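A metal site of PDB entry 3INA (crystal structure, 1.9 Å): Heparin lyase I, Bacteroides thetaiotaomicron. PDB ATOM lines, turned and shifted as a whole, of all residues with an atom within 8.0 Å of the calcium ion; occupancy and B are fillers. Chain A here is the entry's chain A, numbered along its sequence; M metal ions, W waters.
Residues that only touch the calcium ion: Arg 344 (3.996 Å). The nearest printed residue that does not touch the calcium ion is Lys 247 (4.1 Å).
The calcium ion is bound by the backbone carbonyl oxygen (O) of Trp 248 (2.5 Å), the backbone carbonyl oxygen (O) of Asn 345 (2.5 Å), water W1 (2.6 Å), the side-chain carboxylate (OE1) of Glu 222 (2.6 Å) and the side-chain carboxylate (OE2) of Glu 222 (2.7 Å). Slightly farther from the calcium ion lies OD1 of Asp 346 (2.9 Å). Slightly farther from the calcium ion lies water W2 (2.9 Å).
Water W1 lies within hydrogen-bond range of O of Lys 247, OG1 of Thr 250 and OD1 of Asp 346.
The guanidinium group (NH1) of Arg 344 is in salt-bridge range of the side-chain carboxylate (OD2) of Asp 245 (3.98 Å). The guanidinium group of Arg 344 lies within salt-bridge range of the side-chain carboxylate of Asp 346. O of Leu 158 is in hydrogen-bond range of N of Glu 222 (3.1 Å). The side-chain hydroxyl (OG1) of Thr 250 is in hydrogen-bond range of the guanidinium group (NH1) of Arg 344 (3.0 Å). The guanidinium group of Arg 344 sits close to the side-chain carboxylate of Glu 222 (3.1 Å). N of Asn 345 sits at hydrogen-bond distance from O of Asp 245 (2.9 Å). NE2 of Gln 123 lies within hydrogen-bond range of O of Arg 344 (3.0 Å). O of Asp 346 lies close to NE2 of Gln 123.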
ATOM      1  N   GLN A 123     -15.945   0.376  -7.578  1.00  0.00           N
ATOM      2  CA  GLN A 123     -15.397   1.723  -7.492  1.00  0.00           C
ATOM      3  C   GLN A 123     -16.205   2.612  -8.437  1.00  0.00           C
ATOM      4  O   GLN A 123     -16.613   2.180  -9.519  1.00  0.00           O
ATOM      5  CB  GLN A 123     -13.941   1.722  -7.969  1.00  0.00           C
ATOM      6  CG  GLN A 123     -12.918   1.376  -6.911  1.00  0.00           C
ATOM      7  CD  GLN A 123     -12.744   2.501  -5.920  1.00  0.00           C
ATOM      8  OE1 GLN A 123     -12.710   3.671  -6.301  1.00  0.00           O
ATOM      9  NE2 GLN A 123     -12.610   2.160  -4.644  1.00  0.00           N
ATOM     10  N   MET A 153     -12.440  -1.450   0.904  1.00  0.00           N
ATOM     11  CA  MET A 153     -11.816  -2.754   0.790  1.00  0.00           C
ATOM     12  C   MET A 153     -10.399  -2.599   0.258  1.00  0.00           C
ATOM     13  O   MET A 153     -10.160  -2.694  -0.934  1.00  0.00           O
ATOM     14  CB  MET A 153     -12.637  -3.645  -0.136  1.00  0.00           C
ATOM     15  CG  MET A 153     -14.040  -3.867   0.377  1.00  0.00           C
ATOM     16  SD  MET A 153     -15.053  -4.812  -0.775  1.00  0.00           S
ATOM     17  CE  MET A 153     -14.654  -6.494  -0.283  1.00  0.00           C
ATOM     18  N   PRO A 154      -9.448  -2.307   1.155  1.00  0.00           N
ATOM     19  CA  PRO A 154      -8.078  -2.164   0.662  1.00  0.00           C
ATOM     20  C   PRO A 154      -7.431  -3.530   0.460  1.00  0.00           C
ATOM     21  O   PRO A 154      -7.674  -4.462   1.217  1.00  0.00           O
ATOM     22  CB  PRO A 154      -7.407  -1.357   1.772  1.00  0.00           C
ATOM     23  CG  PRO A 154      -8.119  -1.818   2.999  1.00  0.00           C
ATOM     24  CD  PRO A 154      -9.561  -1.892   2.566  1.00  0.00           C
ATOM     25  N   ASP A 155      -6.614  -3.650  -0.579  1.00  0.00           N
ATOM     26  CA  ASP A 155      -5.912  -4.901  -0.864  1.00  0.00           C
ATOM     27  C   ASP A 155      -4.505  -4.729  -0.304  1.00  0.00           C
ATOM     28  O   ASP A 155      -3.764  -3.856  -0.758  1.00  0.00           O
ATOM     29  CB  ASP A 155      -5.862  -5.143  -2.368  1.00  0.00           C
ATOM     30  CG  ASP A 155      -5.429  -6.557  -2.708  1.00  0.00           C
ATOM     31  OD1 ASP A 155      -4.365  -7.000  -2.223  1.00  0.00           O
ATOM     32  OD2 ASP A 155      -6.161  -7.232  -3.471  1.00  0.00           O
ATOM     33  N   LEU A 158      -0.651  -4.147  -1.813  1.00  0.00           N
ATOM     34  CA  LEU A 158      -0.078  -2.839  -2.142  1.00  0.00           C
ATOM     35  C   LEU A 158       0.684  -2.480  -0.871  1.00  0.00           C
ATOM     36  O   LEU A 158       0.080  -2.241   0.181  1.00  0.00           O
ATOM     37  CB  LEU A 158      -1.155  -1.775  -2.413  1.00  0.00           C
ATOM     38  CG  LEU A 158      -0.633  -0.394  -2.827  1.00  0.00           C
ATOM     39  CD1 LEU A 158       0.157  -0.527  -4.120  1.00  0.00           C
ATOM     40  CD2 LEU A 158      -1.786   0.590  -3.022  1.00  0.00           C
ATOM     41  N   GLU A 222      -1.355  -1.867   2.869  1.00  0.00           N
ATOM     42  CA  GLU A 222      -2.553  -1.070   2.952  1.00  0.00           C
ATOM     43  C   GLU A 222      -3.580  -1.834   3.755  1.00  0.00           C
ATOM     44  O   GLU A 222      -3.944  -2.960   3.429  1.00  0.00           O
ATOM     45  CB  GLU A 222      -3.102  -0.715   1.578  1.00  0.00           C
ATOM     46  CG  GLU A 222      -4.306   0.207   1.727  1.00  0.00           C
ATOM     47  CD  GLU A 222      -4.632   0.980   0.491  1.00  0.00           C
ATOM     48  OE1 GLU A 222      -4.853   0.334  -0.554  1.00  0.00           O
ATOM     49  OE2 GLU A 222      -4.670   2.219   0.563  1.00  0.00           O
ATOM     50  N   GLN A 223      -4.069  -1.193   4.819  1.00  0.00           N
ATOM     51  CA  GLN A 223      -5.011  -1.823   5.708  1.00  0.00           C
ATOM     52  C   GLN A 223      -5.779  -0.758   6.474  1.00  0.00           C
ATOM     53  O   GLN A 223      -5.274   0.355   6.673  1.00  0.00           O
ATOM     54  CB  GLN A 223      -4.231  -2.732   6.667  1.00  0.00           C
ATOM     55  CG  GLN A 223      -5.004  -3.405   7.778  1.00  0.00           C
ATOM     56  CD  GLN A 223      -5.333  -2.476   8.923  1.00  0.00           C
ATOM     57  OE1 GLN A 223      -4.660  -1.460   9.137  1.00  0.00           O
ATOM     58  NE2 GLN A 223      -6.361  -2.823   9.692  1.00  0.00           N
ATOM     59  N   ASP A 245     -10.305   9.611   0.388  1.00  0.00           N
ATOM     60  CA  ASP A 245      -8.867   9.413   0.490  1.00  0.00           C
ATOM     61  C   ASP A 245      -8.415   9.137  -0.933  1.00  0.00           C
ATOM     62  O   ASP A 245      -8.699   8.062  -1.467  1.00  0.00           O
ATOM     63  CB  ASP A 245      -8.554   8.206   1.372  1.00  0.00           C
ATOM     64  CG  ASP A 245      -7.074   8.059   1.687  1.00  0.00           C
ATOM     65  OD1 ASP A 245      -6.249   8.705   1.007  1.00  0.00           O
ATOM     66  OD2 ASP A 245      -6.749   7.272   2.610  1.00  0.00           O
ATOM     67  N   ARG A 246      -7.734  10.095  -1.553  1.00  0.00           N
ATOM     68  CA  ARG A 246      -7.283   9.920  -2.938  1.00  0.00           C
ATOM     69  C   ARG A 246      -5.877   9.353  -3.072  1.00  0.00           C
ATOM     70  O   ARG A 246      -5.423   9.077  -4.184  1.00  0.00           O
ATOM     71  CB  ARG A 246      -7.374  11.265  -3.691  1.00  0.00           C
ATOM     72  CG  ARG A 246      -6.301  12.265  -3.291  1.00  0.00           C
ATOM     73  CD  ARG A 246      -6.447  13.610  -3.996  1.00  0.00           C
ATOM     74  NE  ARG A 246      -5.468  14.582  -3.495  1.00  0.00           N
ATOM     75  CZ  ARG A 246      -4.315  14.880  -4.089  1.00  0.00           C
ATOM     76  NH1 ARG A 246      -3.979  14.282  -5.221  1.00  0.00           N
ATOM     77  NH2 ARG A 246      -3.484  15.744  -3.524  1.00  0.00           N
ATOM     78  N   LYS A 247      -5.177   9.161  -1.965  1.00  0.00           N
ATOM     79  CA  LYS A 247      -3.822   8.605  -2.032  1.00  0.00           C
ATOM     80  C   LYS A 247      -3.895   7.140  -2.492  1.00  0.00           C
ATOM     81  O   LYS A 247      -4.814   6.420  -2.096  1.00  0.00           O
ATOM     82  CB  LYS A 247      -3.121   8.703  -0.670  1.00  0.00           C
ATOM     83  CG  LYS A 247      -1.584   8.624  -0.731  1.00  0.00           C
ATOM     84  CD  LYS A 247      -0.959   8.924   0.625  1.00  0.00           C
ATOM     85  CE  LYS A 247       0.563   8.973   0.559  1.00  0.00           C
ATOM     86  NZ  LYS A 247       1.127   7.648   0.175  1.00  0.00           N
ATOM     87  N   TRP A 248      -2.957   6.736  -3.329  1.00  0.00           N
ATOM     88  CA  TRP A 248      -2.933   5.364  -3.845  1.00  0.00           C
ATOM     89  C   TRP A 248      -2.734   4.405  -2.664  1.00  0.00           C
ATOM     90  O   TRP A 248      -3.478   3.444  -2.519  1.00  0.00           O
ATOM     91  CB  TRP A 248      -1.808   5.189  -4.879  1.00  0.00           C
ATOM     92  CG  TRP A 248      -1.750   3.842  -5.567  1.00  0.00           C
ATOM     93  CD1 TRP A 248      -0.642   3.080  -5.800  1.00  0.00           C
ATOM     94  CD2 TRP A 248      -2.864   3.107  -6.124  1.00  0.00           C
ATOM     95  NE1 TRP A 248      -0.980   1.925  -6.461  1.00  0.00           N
ATOM     96  CE2 TRP A 248      -2.331   1.920  -6.677  1.00  0.00           C
ATOM     97  CE3 TRP A 248      -4.232   3.347  -6.213  1.00  0.00           C
ATOM     98  CZ2 TRP A 248      -3.141   0.960  -7.303  1.00  0.00           C
ATOM     99  CZ3 TRP A 248      -5.038   2.403  -6.845  1.00  0.00           C
ATOM    100  CH2 TRP A 248      -4.483   1.216  -7.380  1.00  0.00           C
ATOM    101  N   LEU A 249      -1.715   4.652  -1.843  1.00  0.00           N
ATOM    102  CA  LEU A 249      -1.504   3.828  -0.644  1.00  0.00           C
ATOM    103  C   LEU A 249      -1.879   4.740   0.526  1.00  0.00           C
ATOM    104  O   LEU A 249      -1.217   5.740   0.790  1.00  0.00           O
ATOM    105  CB  LEU A 249      -0.030   3.415  -0.519  1.00  0.00           C
ATOM    106  CG  LEU A 249       0.394   2.885   0.856  1.00  0.00           C
ATOM    107  CD1 LEU A 249      -0.462   1.684   1.239  1.00  0.00           C
ATOM    108  CD2 LEU A 249       1.873   2.496   0.836  1.00  0.00           C
ATOM    109  N   THR A 250      -2.973   4.406   1.207  1.00  0.00           N
ATOM    110  CA  THR A 250      -3.449   5.213   2.324  1.00  0.00           C
ATOM    111  C   THR A 250      -2.414   5.393   3.437  1.00  0.00           C
ATOM    112  O   THR A 250      -1.717   4.454   3.808  1.00  0.00           O
ATOM    113  CB  THR A 250      -4.737   4.612   2.943  1.00  0.00           C
ATOM    114  OG1 THR A 250      -5.850   4.805   2.047  1.00  0.00           O
ATOM    115  CG2 THR A 250      -5.063   5.286   4.283  1.00  0.00           C
ATOM    116  N   ASP A 251      -2.332   6.614   3.943  1.00  0.00           N
ATOM    117  CA  ASP A 251      -1.411   6.979   5.030  1.00  0.00           C
ATOM    118  C   ASP A 251      -2.270   7.030   6.287  1.00  0.00           C
ATOM    119  O   ASP A 251      -3.042   7.970   6.477  1.00  0.00           O
ATOM    120  CB  ASP A 251      -0.831   8.369   4.739  1.00  0.00           C
ATOM    121  CG  ASP A 251       0.066   8.880   5.844  1.00  0.00           C
ATOM    122  OD1 ASP A 251       0.317   8.159   6.842  1.00  0.00           O
ATOM    123  OD2 ASP A 251       0.544  10.021   5.720  1.00  0.00           O
ATOM    124  N   LYS A 306      -6.346   6.210  -9.534  1.00  0.00           N
ATOM    125  CA  LYS A 306      -5.390   5.164  -9.198  1.00  0.00           C
ATOM    126  C   LYS A 306      -3.974   5.656  -8.870  1.00  0.00           C
ATOM    127  O   LYS A 306      -3.782   6.466  -7.973  1.00  0.00           O
ATOM    128  CB  LYS A 306      -5.349   4.146 -10.329  1.00  0.00           C
ATOM    129  CG  LYS A 306      -6.710   3.518 -10.624  1.00  0.00           C
ATOM    130  CD  LYS A 306      -6.605   2.424 -11.675  1.00  0.00           C
ATOM    131  CE  LYS A 306      -7.962   1.820 -11.985  1.00  0.00           C
ATOM    132  NZ  LYS A 306      -8.609   1.221 -10.784  1.00  0.00           N
ATOM    133  N   ARG A 344     -12.595   5.810  -1.490  1.00  0.00           N
ATOM    134  CA  ARG A 344     -11.164   5.541  -1.309  1.00  0.00           C
ATOM    135  C   ARG A 344     -10.547   5.165  -2.656  1.00  0.00           C
ATOM    136  O   ARG A 344     -11.173   4.495  -3.465  1.00  0.00           O
ATOM    137  CB  ARG A 344     -10.931   4.343  -0.369  1.00  0.00           C
ATOM    138  CG  ARG A 344     -11.273   4.554   1.096  1.00  0.00           C
ATOM    139  CD  ARG A 344     -11.153   3.216   1.834  1.00  0.00           C
ATOM    140  NE  ARG A 344      -9.924   2.529   1.456  1.00  0.00           N
ATOM    141  CZ  ARG A 344      -8.718   2.793   1.963  1.00  0.00           C
ATOM    142  NH1 ARG A 344      -8.566   3.737   2.889  1.00  0.00           N
ATOM    143  NH2 ARG A 344      -7.651   2.125   1.516  1.00  0.00           N
ATOM    144  N   ASN A 345      -9.305   5.587  -2.880  1.00  0.00           N
ATOM    145  CA  ASN A 345      -8.624   5.274  -4.124  1.00  0.00           C
ATOM    146  C   ASN A 345      -8.068   3.862  -4.022  1.00  0.00           C
ATOM    147  O   ASN A 345      -6.889   3.680  -3.767  1.00  0.00           O
ATOM    148  CB  ASN A 345      -7.491   6.284  -4.357  1.00  0.00           C
ATOM    149  CG  ASN A 345      -6.757   6.029  -5.648  1.00  0.00           C
ATOM    150  OD1 ASN A 345      -7.174   5.224  -6.485  1.00  0.00           O
ATOM    151  ND2 ASN A 345      -5.648   6.732  -5.837  1.00  0.00           N
ATOM    152  N   ASP A 346      -8.937   2.879  -4.235  1.00  0.00           N
ATOM    153  CA  ASP A 346      -8.581   1.457  -4.186  1.00  0.00           C
ATOM    154  C   ASP A 346      -9.039   0.794  -5.482  1.00  0.00           C
ATOM    155  O   ASP A 346      -9.774   1.392  -6.266  1.00  0.00           O
ATOM    156  CB  ASP A 346      -9.326   0.729  -3.067  1.00  0.00           C
ATOM    157  CG  ASP A 346      -9.122   1.343  -1.709  1.00  0.00           C
ATOM    158  OD1 ASP A 346      -8.546   2.446  -1.612  1.00  0.00           O
ATOM    159  OD2 ASP A 346      -9.571   0.730  -0.719  1.00  0.00           O
ATOM    160  N   GLU A 347      -8.627  -0.453  -5.667  1.00  0.00           N
ATOM    161  CA  GLU A 347      -9.051  -1.203  -6.843  1.00  0.00           C
ATOM    162  C   GLU A 347     -10.493  -1.679  -6.580  1.00  0.00           C
ATOM    163  O   GLU A 347     -11.339  -1.626  -7.475  1.00  0.00           O
ATOM    164  CB  GLU A 347      -8.135  -2.416  -7.069  1.00  0.00           C
ATOM    165  CG  GLU A 347      -6.757  -2.075  -7.621  1.00  0.00           C
ATOM    166  CD  GLU A 347      -6.788  -1.635  -9.077  1.00  0.00           C
ATOM    167  OE1 GLU A 347      -5.709  -1.325  -9.622  1.00  0.00           O
ATOM    168  OE2 GLU A 347      -7.896  -1.613  -9.666  1.00  0.00           O
ATOM    169  N   ASP A 348     -10.757  -2.127  -5.354  1.00  0.00           N
ATOM    170  CA  ASP A 348     -12.086  -2.611  -4.995  1.00  0.00           C
ATOM    171  C   ASP A 348     -13.019  -1.561  -4.398  1.00  0.00           C
ATOM    172  O   ASP A 348     -12.589  -0.482  -3.996  1.00  0.00           O
ATOM    173  CB  ASP A 348     -11.990  -3.794  -4.028  1.00  0.00           C
ATOM    174  CG  ASP A 348     -11.334  -5.003  -4.659  1.00  0.00           C
ATOM    175  OD1 ASP A 348     -11.669  -5.319  -5.823  1.00  0.00           O
ATOM    176  OD2 ASP A 348     -10.500  -5.649  -3.991  1.00  0.00           O
HETATM  177 CA    CA M   1      -5.658   2.427  -1.934  1.00  0.00          CA
HETATM  178  O   HOH W   1      -6.362   4.587  -0.708  1.00  0.00           O
HETATM  179  O   HOH W   2      -4.918   0.822  -4.250  1.00  0.00           O
